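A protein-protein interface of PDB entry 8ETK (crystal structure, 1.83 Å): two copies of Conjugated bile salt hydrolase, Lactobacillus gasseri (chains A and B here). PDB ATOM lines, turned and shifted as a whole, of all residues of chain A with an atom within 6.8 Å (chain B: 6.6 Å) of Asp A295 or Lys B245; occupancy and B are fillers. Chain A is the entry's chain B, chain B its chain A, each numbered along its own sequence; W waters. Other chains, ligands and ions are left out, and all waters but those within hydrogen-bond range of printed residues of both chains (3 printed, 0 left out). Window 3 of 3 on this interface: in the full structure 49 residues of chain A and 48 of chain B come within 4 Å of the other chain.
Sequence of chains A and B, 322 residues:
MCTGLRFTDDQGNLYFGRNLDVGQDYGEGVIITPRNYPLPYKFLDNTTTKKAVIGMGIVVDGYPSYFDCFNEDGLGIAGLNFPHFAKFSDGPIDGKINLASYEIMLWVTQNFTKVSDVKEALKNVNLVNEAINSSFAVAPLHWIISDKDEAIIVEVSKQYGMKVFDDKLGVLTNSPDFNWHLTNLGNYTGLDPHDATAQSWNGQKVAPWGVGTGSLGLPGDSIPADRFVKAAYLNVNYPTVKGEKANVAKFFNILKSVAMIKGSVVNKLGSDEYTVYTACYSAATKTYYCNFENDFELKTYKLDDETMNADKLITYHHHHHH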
ATOM      1  N   CYS A 290       4.207  -4.140  18.629  1.00  0.00           N
ATOM      2  CA  CYS A 290       3.039  -3.874  17.797  1.00  0.00           C
ATOM      3  C   CYS A 290       2.198  -5.129  17.612  1.00  0.00           C
ATOM      4  O   CYS A 290       2.688  -6.254  17.747  1.00  0.00           O
ATOM      5  CB  CYS A 290       3.436  -3.297  16.437  1.00  0.00           C
ATOM      6  SG  CYS A 290       4.572  -4.351  15.488  1.00  0.00           S
ATOM      7  N   ASN A 291       0.902  -4.925  17.346  1.00  0.00           N
ATOM      8  CA  ASN A 291       0.076  -5.990  16.805  1.00  0.00           C
ATOM      9  C   ASN A 291      -0.791  -5.407  15.698  1.00  0.00           C
ATOM     10  O   ASN A 291      -0.746  -4.207  15.415  1.00  0.00           O
ATOM     11  CB  ASN A 291      -0.707  -6.730  17.919  1.00  0.00           C
ATOM     12  CG  ASN A 291      -1.920  -5.957  18.466  1.00  0.00           C
ATOM     13  OD1 ASN A 291      -2.147  -4.790  18.157  1.00  0.00           O
ATOM     14  ND2 ASN A 291      -2.682  -6.628  19.331  1.00  0.00           N
ATOM     15  N   PHE A 292      -1.552  -6.274  15.039  1.00  0.00           N
ATOM     16  CA  PHE A 292      -2.238  -5.940  13.800  1.00  0.00           C
ATOM     17  C   PHE A 292      -3.682  -6.397  13.855  1.00  0.00           C
ATOM     18  O   PHE A 292      -4.056  -7.232  14.686  1.00  0.00           O
ATOM     19  CB  PHE A 292      -1.528  -6.575  12.594  1.00  0.00           C
ATOM     20  CG  PHE A 292      -0.136  -6.062  12.411  1.00  0.00           C
ATOM     21  CD1 PHE A 292       0.914  -6.590  13.145  1.00  0.00           C
ATOM     22  CD2 PHE A 292       0.116  -5.011  11.554  1.00  0.00           C
ATOM     23  CE1 PHE A 292       2.194  -6.092  13.002  1.00  0.00           C
ATOM     24  CE2 PHE A 292       1.392  -4.509  11.416  1.00  0.00           C
ATOM     25  CZ  PHE A 292       2.428  -5.051  12.142  1.00  0.00           C
ATOM     26  N   GLU A 293      -4.487  -5.859  12.928  1.00  0.00           N
ATOM     27  CA  GLU A 293      -5.914  -6.172  12.917  1.00  0.00           C
ATOM     28  C   GLU A 293      -6.168  -7.664  12.783  1.00  0.00           C
ATOM     29  O   GLU A 293      -7.146  -8.183  13.343  1.00  0.00           O
ATOM     30  CB  GLU A 293      -6.623  -5.426  11.782  1.00  0.00           C
ATOM     31  CG  GLU A 293      -8.132  -5.676  11.697  1.00  0.00           C
ATOM     32  CD  GLU A 293      -8.516  -6.930  10.906  1.00  0.00           C
ATOM     33  OE1 GLU A 293      -7.721  -7.368  10.059  1.00  0.00           O
ATOM     34  OE2 GLU A 293      -9.616  -7.493  11.143  1.00  0.00           O
ATOM     35  N   ASN A 294      -5.325  -8.376  12.031  1.00  0.00           N
ATOM     36  CA  ASN A 294      -5.555  -9.800  11.809  1.00  0.00           C
ATOM     37  C   ASN A 294      -4.518 -10.672  12.507  1.00  0.00           C
ATOM     38  O   ASN A 294      -4.425 -11.865  12.208  1.00  0.00           O
ATOM     39  CB  ASN A 294      -5.599 -10.108  10.310  1.00  0.00           C
ATOM     40  CG  ASN A 294      -4.293  -9.792   9.612  1.00  0.00           C
ATOM     41  OD1 ASN A 294      -3.378  -9.213  10.209  1.00  0.00           O
ATOM     42  ND2 ASN A 294      -4.195 -10.165   8.339  1.00  0.00           N
ATOM     43  N   ASP A 295      -3.739 -10.109  13.436  1.00  0.00           N
ATOM     44  CA  ASP A 295      -2.772 -10.905  14.200  1.00  0.00           C
ATOM     45  C   ASP A 295      -2.548 -10.193  15.532  1.00  0.00           C
ATOM     46  O   ASP A 295      -1.822  -9.197  15.585  1.00  0.00           O
ATOM     47  CB  ASP A 295      -1.472 -11.087  13.418  1.00  0.00           C
ATOM     48  CG  ASP A 295      -0.484 -12.034  14.106  1.00  0.00           C
ATOM     49  OD1 ASP A 295      -0.703 -12.410  15.281  1.00  0.00           O
ATOM     50  OD2 ASP A 295       0.527 -12.398  13.464  1.00  0.00           O
ATOM     51  N   PHE A 296      -3.165 -10.716  16.602  1.00  0.00           N
ATOM     52  CA  PHE A 296      -3.261  -9.985  17.864  1.00  0.00           C
ATOM     53  C   PHE A 296      -2.057 -10.181  18.779  1.00  0.00           C
ATOM     54  O   PHE A 296      -1.850  -9.373  19.698  1.00  0.00           O
ATOM     55  CB  PHE A 296      -4.553 -10.384  18.598  1.00  0.00           C
ATOM     56  CG  PHE A 296      -5.094  -9.301  19.510  1.00  0.00           C
ATOM     57  CD1 PHE A 296      -5.883  -8.279  19.006  1.00  0.00           C
ATOM     58  CD2 PHE A 296      -4.787  -9.301  20.862  1.00  0.00           C
ATOM     59  CE1 PHE A 296      -6.368  -7.275  19.842  1.00  0.00           C
ATOM     60  CE2 PHE A 296      -5.277  -8.306  21.707  1.00  0.00           C
ATOM     61  CZ  PHE A 296      -6.058  -7.288  21.194  1.00  0.00           C
ATOM     62  N   GLU A 297      -1.249 -11.214  18.554  1.00  0.00           N
ATOM     63  CA  GLU A 297      -0.077 -11.426  19.389  1.00  0.00           C
ATOM     64  C   GLU A 297       0.895 -10.257  19.246  1.00  0.00           C
ATOM     65  O   GLU A 297       1.060  -9.700  18.160  1.00  0.00           O
ATOM     66  CB  GLU A 297       0.603 -12.747  19.009  1.00  0.00           C
ATOM     67  N   LEU A 298       1.511  -9.857  20.358  1.00  0.00           N
ATOM     68  CA  LEU A 298       2.460  -8.753  20.334  1.00  0.00           C
ATOM     69  C   LEU A 298       3.773  -9.202  19.697  1.00  0.00           C
ATOM     70  O   LEU A 298       4.359 -10.203  20.117  1.00  0.00           O
ATOM     71  CB  LEU A 298       2.732  -8.240  21.751  1.00  0.00           C
ATOM     72  CG  LEU A 298       1.603  -7.553  22.538  1.00  0.00           C
ATOM     73  CD1 LEU A 298       2.160  -6.825  23.757  1.00  0.00           C
ATOM     74  CD2 LEU A 298       0.804  -6.600  21.667  1.00  0.00           C
ATOM     75  N   LYS A 299       4.234  -8.465  18.692  1.00  0.00           N
ATOM     76  CA  LYS A 299       5.562  -8.667  18.125  1.00  0.00           C
ATOM     77  C   LYS A 299       6.498  -7.576  18.629  1.00  0.00           C
ATOM     78  O   LYS A 299       6.072  -6.445  18.889  1.00  0.00           O
ATOM     79  CB  LYS A 299       5.518  -8.654  16.597  1.00  0.00           C
ATOM     80  CG  LYS A 299       4.318  -9.357  16.038  1.00  0.00           C
ATOM     81  CD  LYS A 299       4.704 -10.445  15.059  1.00  0.00           C
ATOM     82  CE  LYS A 299       3.605 -11.502  14.964  1.00  0.00           C
ATOM     83  N   TYR B  15     -15.948 -19.030  17.515  1.00  0.00           N
ATOM     84  CA  TYR B  15     -15.108 -18.246  18.407  1.00  0.00           C
ATOM     85  C   TYR B  15     -16.037 -17.620  19.445  1.00  0.00           C
ATOM     86  O   TYR B  15     -16.972 -16.902  19.080  1.00  0.00           O
ATOM     87  CB  TYR B  15     -14.316 -17.201  17.611  1.00  0.00           C
ATOM     88  CG  TYR B  15     -13.361 -17.901  16.659  1.00  0.00           C
ATOM     89  CD1 TYR B  15     -13.794 -18.369  15.425  1.00  0.00           C
ATOM     90  CD2 TYR B  15     -12.050 -18.168  17.040  1.00  0.00           C
ATOM     91  CE1 TYR B  15     -12.919 -19.057  14.570  1.00  0.00           C
ATOM     92  CE2 TYR B  15     -11.177 -18.855  16.194  1.00  0.00           C
ATOM     93  CZ  TYR B  15     -11.627 -19.296  14.960  1.00  0.00           C
ATOM     94  OH  TYR B  15     -10.749 -19.972  14.122  1.00  0.00           O
ATOM     95  N   LYS B 242     -11.011 -15.148   7.786  1.00  0.00           N
ATOM     96  CA  LYS B 242     -10.566 -16.503   7.470  1.00  0.00           C
ATOM     97  C   LYS B 242      -9.344 -16.871   8.295  1.00  0.00           C
ATOM     98  O   LYS B 242      -8.403 -16.081   8.403  1.00  0.00           O
ATOM     99  CB  LYS B 242     -10.241 -16.644   5.971  1.00  0.00           C
ATOM    100  N   GLY B 243      -9.355 -18.071   8.862  1.00  0.00           N
ATOM    101  CA  GLY B 243      -8.142 -18.514   9.542  1.00  0.00           C
ATOM    102  C   GLY B 243      -8.173 -18.240  11.034  1.00  0.00           C
ATOM    103  O   GLY B 243      -8.805 -17.297  11.517  1.00  0.00           O
ATOM    104  N   GLU B 244      -7.449 -19.081  11.776  1.00  0.00           N
ATOM    105  CA  GLU B 244      -7.469 -19.016  13.236  1.00  0.00           C
ATOM    106  C   GLU B 244      -6.917 -17.691  13.747  1.00  0.00           C
ATOM    107  O   GLU B 244      -7.506 -17.061  14.632  1.00  0.00           O
ATOM    108  CB  GLU B 244      -6.668 -20.187  13.806  1.00  0.00           C
ATOM    109  CG  GLU B 244      -6.477 -20.151  15.307  1.00  0.00           C
ATOM    110  CD  GLU B 244      -7.600 -20.822  16.070  1.00  0.00           C
ATOM    111  OE1 GLU B 244      -8.680 -21.056  15.492  1.00  0.00           O
ATOM    112  OE2 GLU B 244      -7.379 -21.151  17.255  1.00  0.00           O
ATOM    113  N   LYS B 245      -5.771 -17.258  13.217  1.00  0.00           N
ATOM    114  CA  LYS B 245      -5.172 -16.013  13.687  1.00  0.00           C
ATOM    115  C   LYS B 245      -6.090 -14.817  13.461  1.00  0.00           C
ATOM    116  O   LYS B 245      -6.191 -13.932  14.326  1.00  0.00           O
ATOM    117  CB  LYS B 245      -3.835 -15.768  12.992  1.00  0.00           C
ATOM    118  CG  LYS B 245      -2.641 -15.922  13.892  1.00  0.00           C
ATOM    119  CD  LYS B 245      -1.468 -16.437  13.117  1.00  0.00           C
ATOM    120  CE  LYS B 245      -0.795 -15.285  12.414  1.00  0.00           C
ATOM    121  N   ALA B 246      -6.718 -14.736  12.283  1.00  0.00           N
ATOM    122  CA  ALA B 246      -7.532 -13.560  11.975  1.00  0.00           C
ATOM    123  C   ALA B 246      -8.810 -13.543  12.802  1.00  0.00           C
ATOM    124  O   ALA B 246      -9.294 -12.469  13.184  1.00  0.00           O
ATOM    125  CB  ALA B 246      -7.869 -13.503  10.483  1.00  0.00           C
ATOM    126  N   ASN B 247      -9.386 -14.716  13.066  1.00  0.00           N
ATOM    127  CA  ASN B 247     -10.627 -14.772  13.839  1.00  0.00           C
ATOM    128  C   ASN B 247     -10.389 -14.491  15.320  1.00  0.00           C
ATOM    129  O   ASN B 247     -11.171 -13.772  15.955  1.00  0.00           O
ATOM    130  CB  ASN B 247     -11.285 -16.129  13.652  1.00  0.00           C
ATOM    131  CG  ASN B 247     -12.151 -16.173  12.427  1.00  0.00           C
ATOM    132  OD1 ASN B 247     -13.297 -15.736  12.458  1.00  0.00           O
ATOM    133  ND2 ASN B 247     -11.605 -16.683  11.328  1.00  0.00           N
ATOM    134  N   VAL B 248      -9.328 -15.056  15.892  1.00  0.00           N
ATOM    135  CA  VAL B 248      -8.946 -14.711  17.260  1.00  0.00           C
ATOM    136  C   VAL B 248      -8.681 -13.212  17.372  1.00  0.00           C
ATOM    137  O   VAL B 248      -9.157 -12.547  18.300  1.00  0.00           O
ATOM    138  CB  VAL B 248      -7.720 -15.537  17.699  1.00  0.00           C
ATOM    139  CG1 VAL B 248      -7.149 -15.007  19.027  1.00  0.00           C
ATOM    140  CG2 VAL B 248      -8.111 -17.006  17.836  1.00  0.00           C
ATOM    141  N   ALA B 249      -7.917 -12.656  16.424  1.00  0.00           N
ATOM    142  CA  ALA B 249      -7.640 -11.223  16.470  1.00  0.00           C
ATOM    143  C   ALA B 249      -8.933 -10.419  16.344  1.00  0.00           C
ATOM    144  O   ALA B 249      -9.135  -9.445  17.076  1.00  0.00           O
ATOM    145  CB  ALA B 249      -6.642 -10.826  15.374  1.00  0.00           C
ATOM    146  N   LYS B 250      -9.816 -10.817  15.428  1.00  0.00           N
ATOM    147  CA  LYS B 250     -11.112 -10.155  15.300  1.00  0.00           C
ATOM    148  C   LYS B 250     -11.877 -10.177  16.624  1.00  0.00           C
ATOM    149  O   LYS B 250     -12.498  -9.180  17.018  1.00  0.00           O
ATOM    150  CB  LYS B 250     -11.929 -10.831  14.205  1.00  0.00           C
ATOM    151  CG  LYS B 250     -13.449 -10.581  14.292  1.00  0.00           C
ATOM    152  CD  LYS B 250     -14.188 -11.321  13.179  1.00  0.00           C
ATOM    153  CE  LYS B 250     -15.688 -11.172  13.329  1.00  0.00           C
ATOM    154  NZ  LYS B 250     -16.441 -11.799  12.209  1.00  0.00           N
ATOM    155  N   ASN B 253     -10.269  -7.766  19.034  1.00  0.00           N
ATOM    156  CA  ASN B 253     -10.522  -6.400  18.581  1.00  0.00           C
ATOM    157  C   ASN B 253     -11.869  -5.902  19.102  1.00  0.00           C
ATOM    158  O   ASN B 253     -11.976  -4.791  19.636  1.00  0.00           O
ATOM    159  CB  ASN B 253     -10.504  -6.331  17.050  1.00  0.00           C
ATOM    160  CG  ASN B 253      -9.122  -6.573  16.451  1.00  0.00           C
ATOM    161  OD1 ASN B 253      -8.091  -6.323  17.072  1.00  0.00           O
ATOM    162  ND2 ASN B 253      -9.110  -7.066  15.226  1.00  0.00           N
ATOM    163  N   TYR B 289      -7.748 -18.994  24.579  1.00  0.00           N
ATOM    164  CA  TYR B 289      -6.872 -17.828  24.545  1.00  0.00           C
ATOM    165  C   TYR B 289      -7.323 -16.802  25.576  1.00  0.00           C
ATOM    166  O   TYR B 289      -8.514 -16.536  25.697  1.00  0.00           O
ATOM    167  CB  TYR B 289      -6.904 -17.127  23.184  1.00  0.00           C
ATOM    168  CG  TYR B 289      -6.523 -17.934  21.970  1.00  0.00           C
ATOM    169  CD1 TYR B 289      -7.421 -18.810  21.382  1.00  0.00           C
ATOM    170  CD2 TYR B 289      -5.277 -17.760  21.368  1.00  0.00           C
ATOM    171  CE1 TYR B 289      -7.077 -19.538  20.246  1.00  0.00           C
ATOM    172  CE2 TYR B 289      -4.922 -18.486  20.230  1.00  0.00           C
ATOM    173  CZ  TYR B 289      -5.824 -19.363  19.682  1.00  0.00           C
ATOM    174  OH  TYR B 289      -5.485 -20.080  18.552  1.00  0.00           O
HETATM  175  O   HOH W   1      -4.416 -13.337  16.508  1.00  0.00           O
HETATM  176  O   HOH W   2      -9.061 -10.265  11.254  1.00  0.00           O
HETATM  177  O   HOH W   3      -5.423  -5.772  16.485  1.00  0.00           O
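Water W3 lies within hydrogen-bond range of O of Phe A292 (2.7 Å) and OD1 of Asn B253 (2.8 Å). Water W2 bridges the side-chain carboxylate (OE2) of Glu A293 (2.8 Å) and the backbone carbonyl oxygen (O) of Ala B246 (2.9 Å). Water W1 lies within hydrogen-bond range of the backbone carbonyl oxygen of Lys B245 (2.9 Å) and the backbone NH of Phe A296 (2.9 Å).
The backbone carbonyl oxygen (O) of Glu A293 is in hydrogen-bond range of the side-chain amide nitrogen (ND2) of Asn B253. The backbone carbonyl oxygen of Asn A294 sits close to the backbone carbonyl oxygen of Lys B245, at 3.4 Å.
Hydrophobic or aromatic side chains of chain B that line the printed part of chain A: Ala B249. Among the printed residues, no Asp or Glu carboxylate lies within 4 Å of a Lys or Arg side-chain nitrogen of the other chain.
Of the printed residues of chain B, Asp A295 touches Lys B245 (3.3 Å) and Ala B249 (3.6 Å). Lys B245 touches just these residues of chain A: Asn A294 (3.4 Å) and Asp A295 (3.3 Å). Of the printed residues of chain A, Ala B246 touches Asn A294. Of the printed residues of chain B, Glu A293 touches Ala B249 (3.4 Å) and Asn B253 (2.9 Å). Of the printed residues of chain B, Asn A294 touches Lys B245 (3.4 Å), Ala B246 (3.5 Å) and Ala B249 (3.6 Å). Printed residues of chain B within 4 Å of Phe A296: Ala B249 and Asn B253. Asn B247 touches none of the printed residues of chain A. Glu A297 touches none of the printed residues of chain B. The nearest residue of chain B that does not touch Asp A295 is Ala B246 (5.3 Å).
The backbone carbonyl oxygen (O) of Ala B249 lies close to the side-chain amide nitrogen (ND2) of Asn B253 (3.0 Å). The side-chain amide nitrogen (ND2) of Asn A291 is in hydrogen-bond range of the backbone carbonyl oxygen (O) of Phe A296 (2.9 Å).
Glu A293 touches Ala B249. Asn A294 touches Ala B246. C of Asn A294 touches CB of Ala B249, 3.6 Å away. Asp A295 touches Lys B245 (OD2 to CE, 3.3 Å). Ala B249 touches Asp A295. Phe A296 touches Ala B249 (N to CB, 3.7 Å). Phe A296 touches Asn B253 (CE1 to OD1, 3.4 Å).
No position is printed for both chains. Of the 9 pairs that touch across the chains among the printed residues, none has its exchanged pair printed and touching as well.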
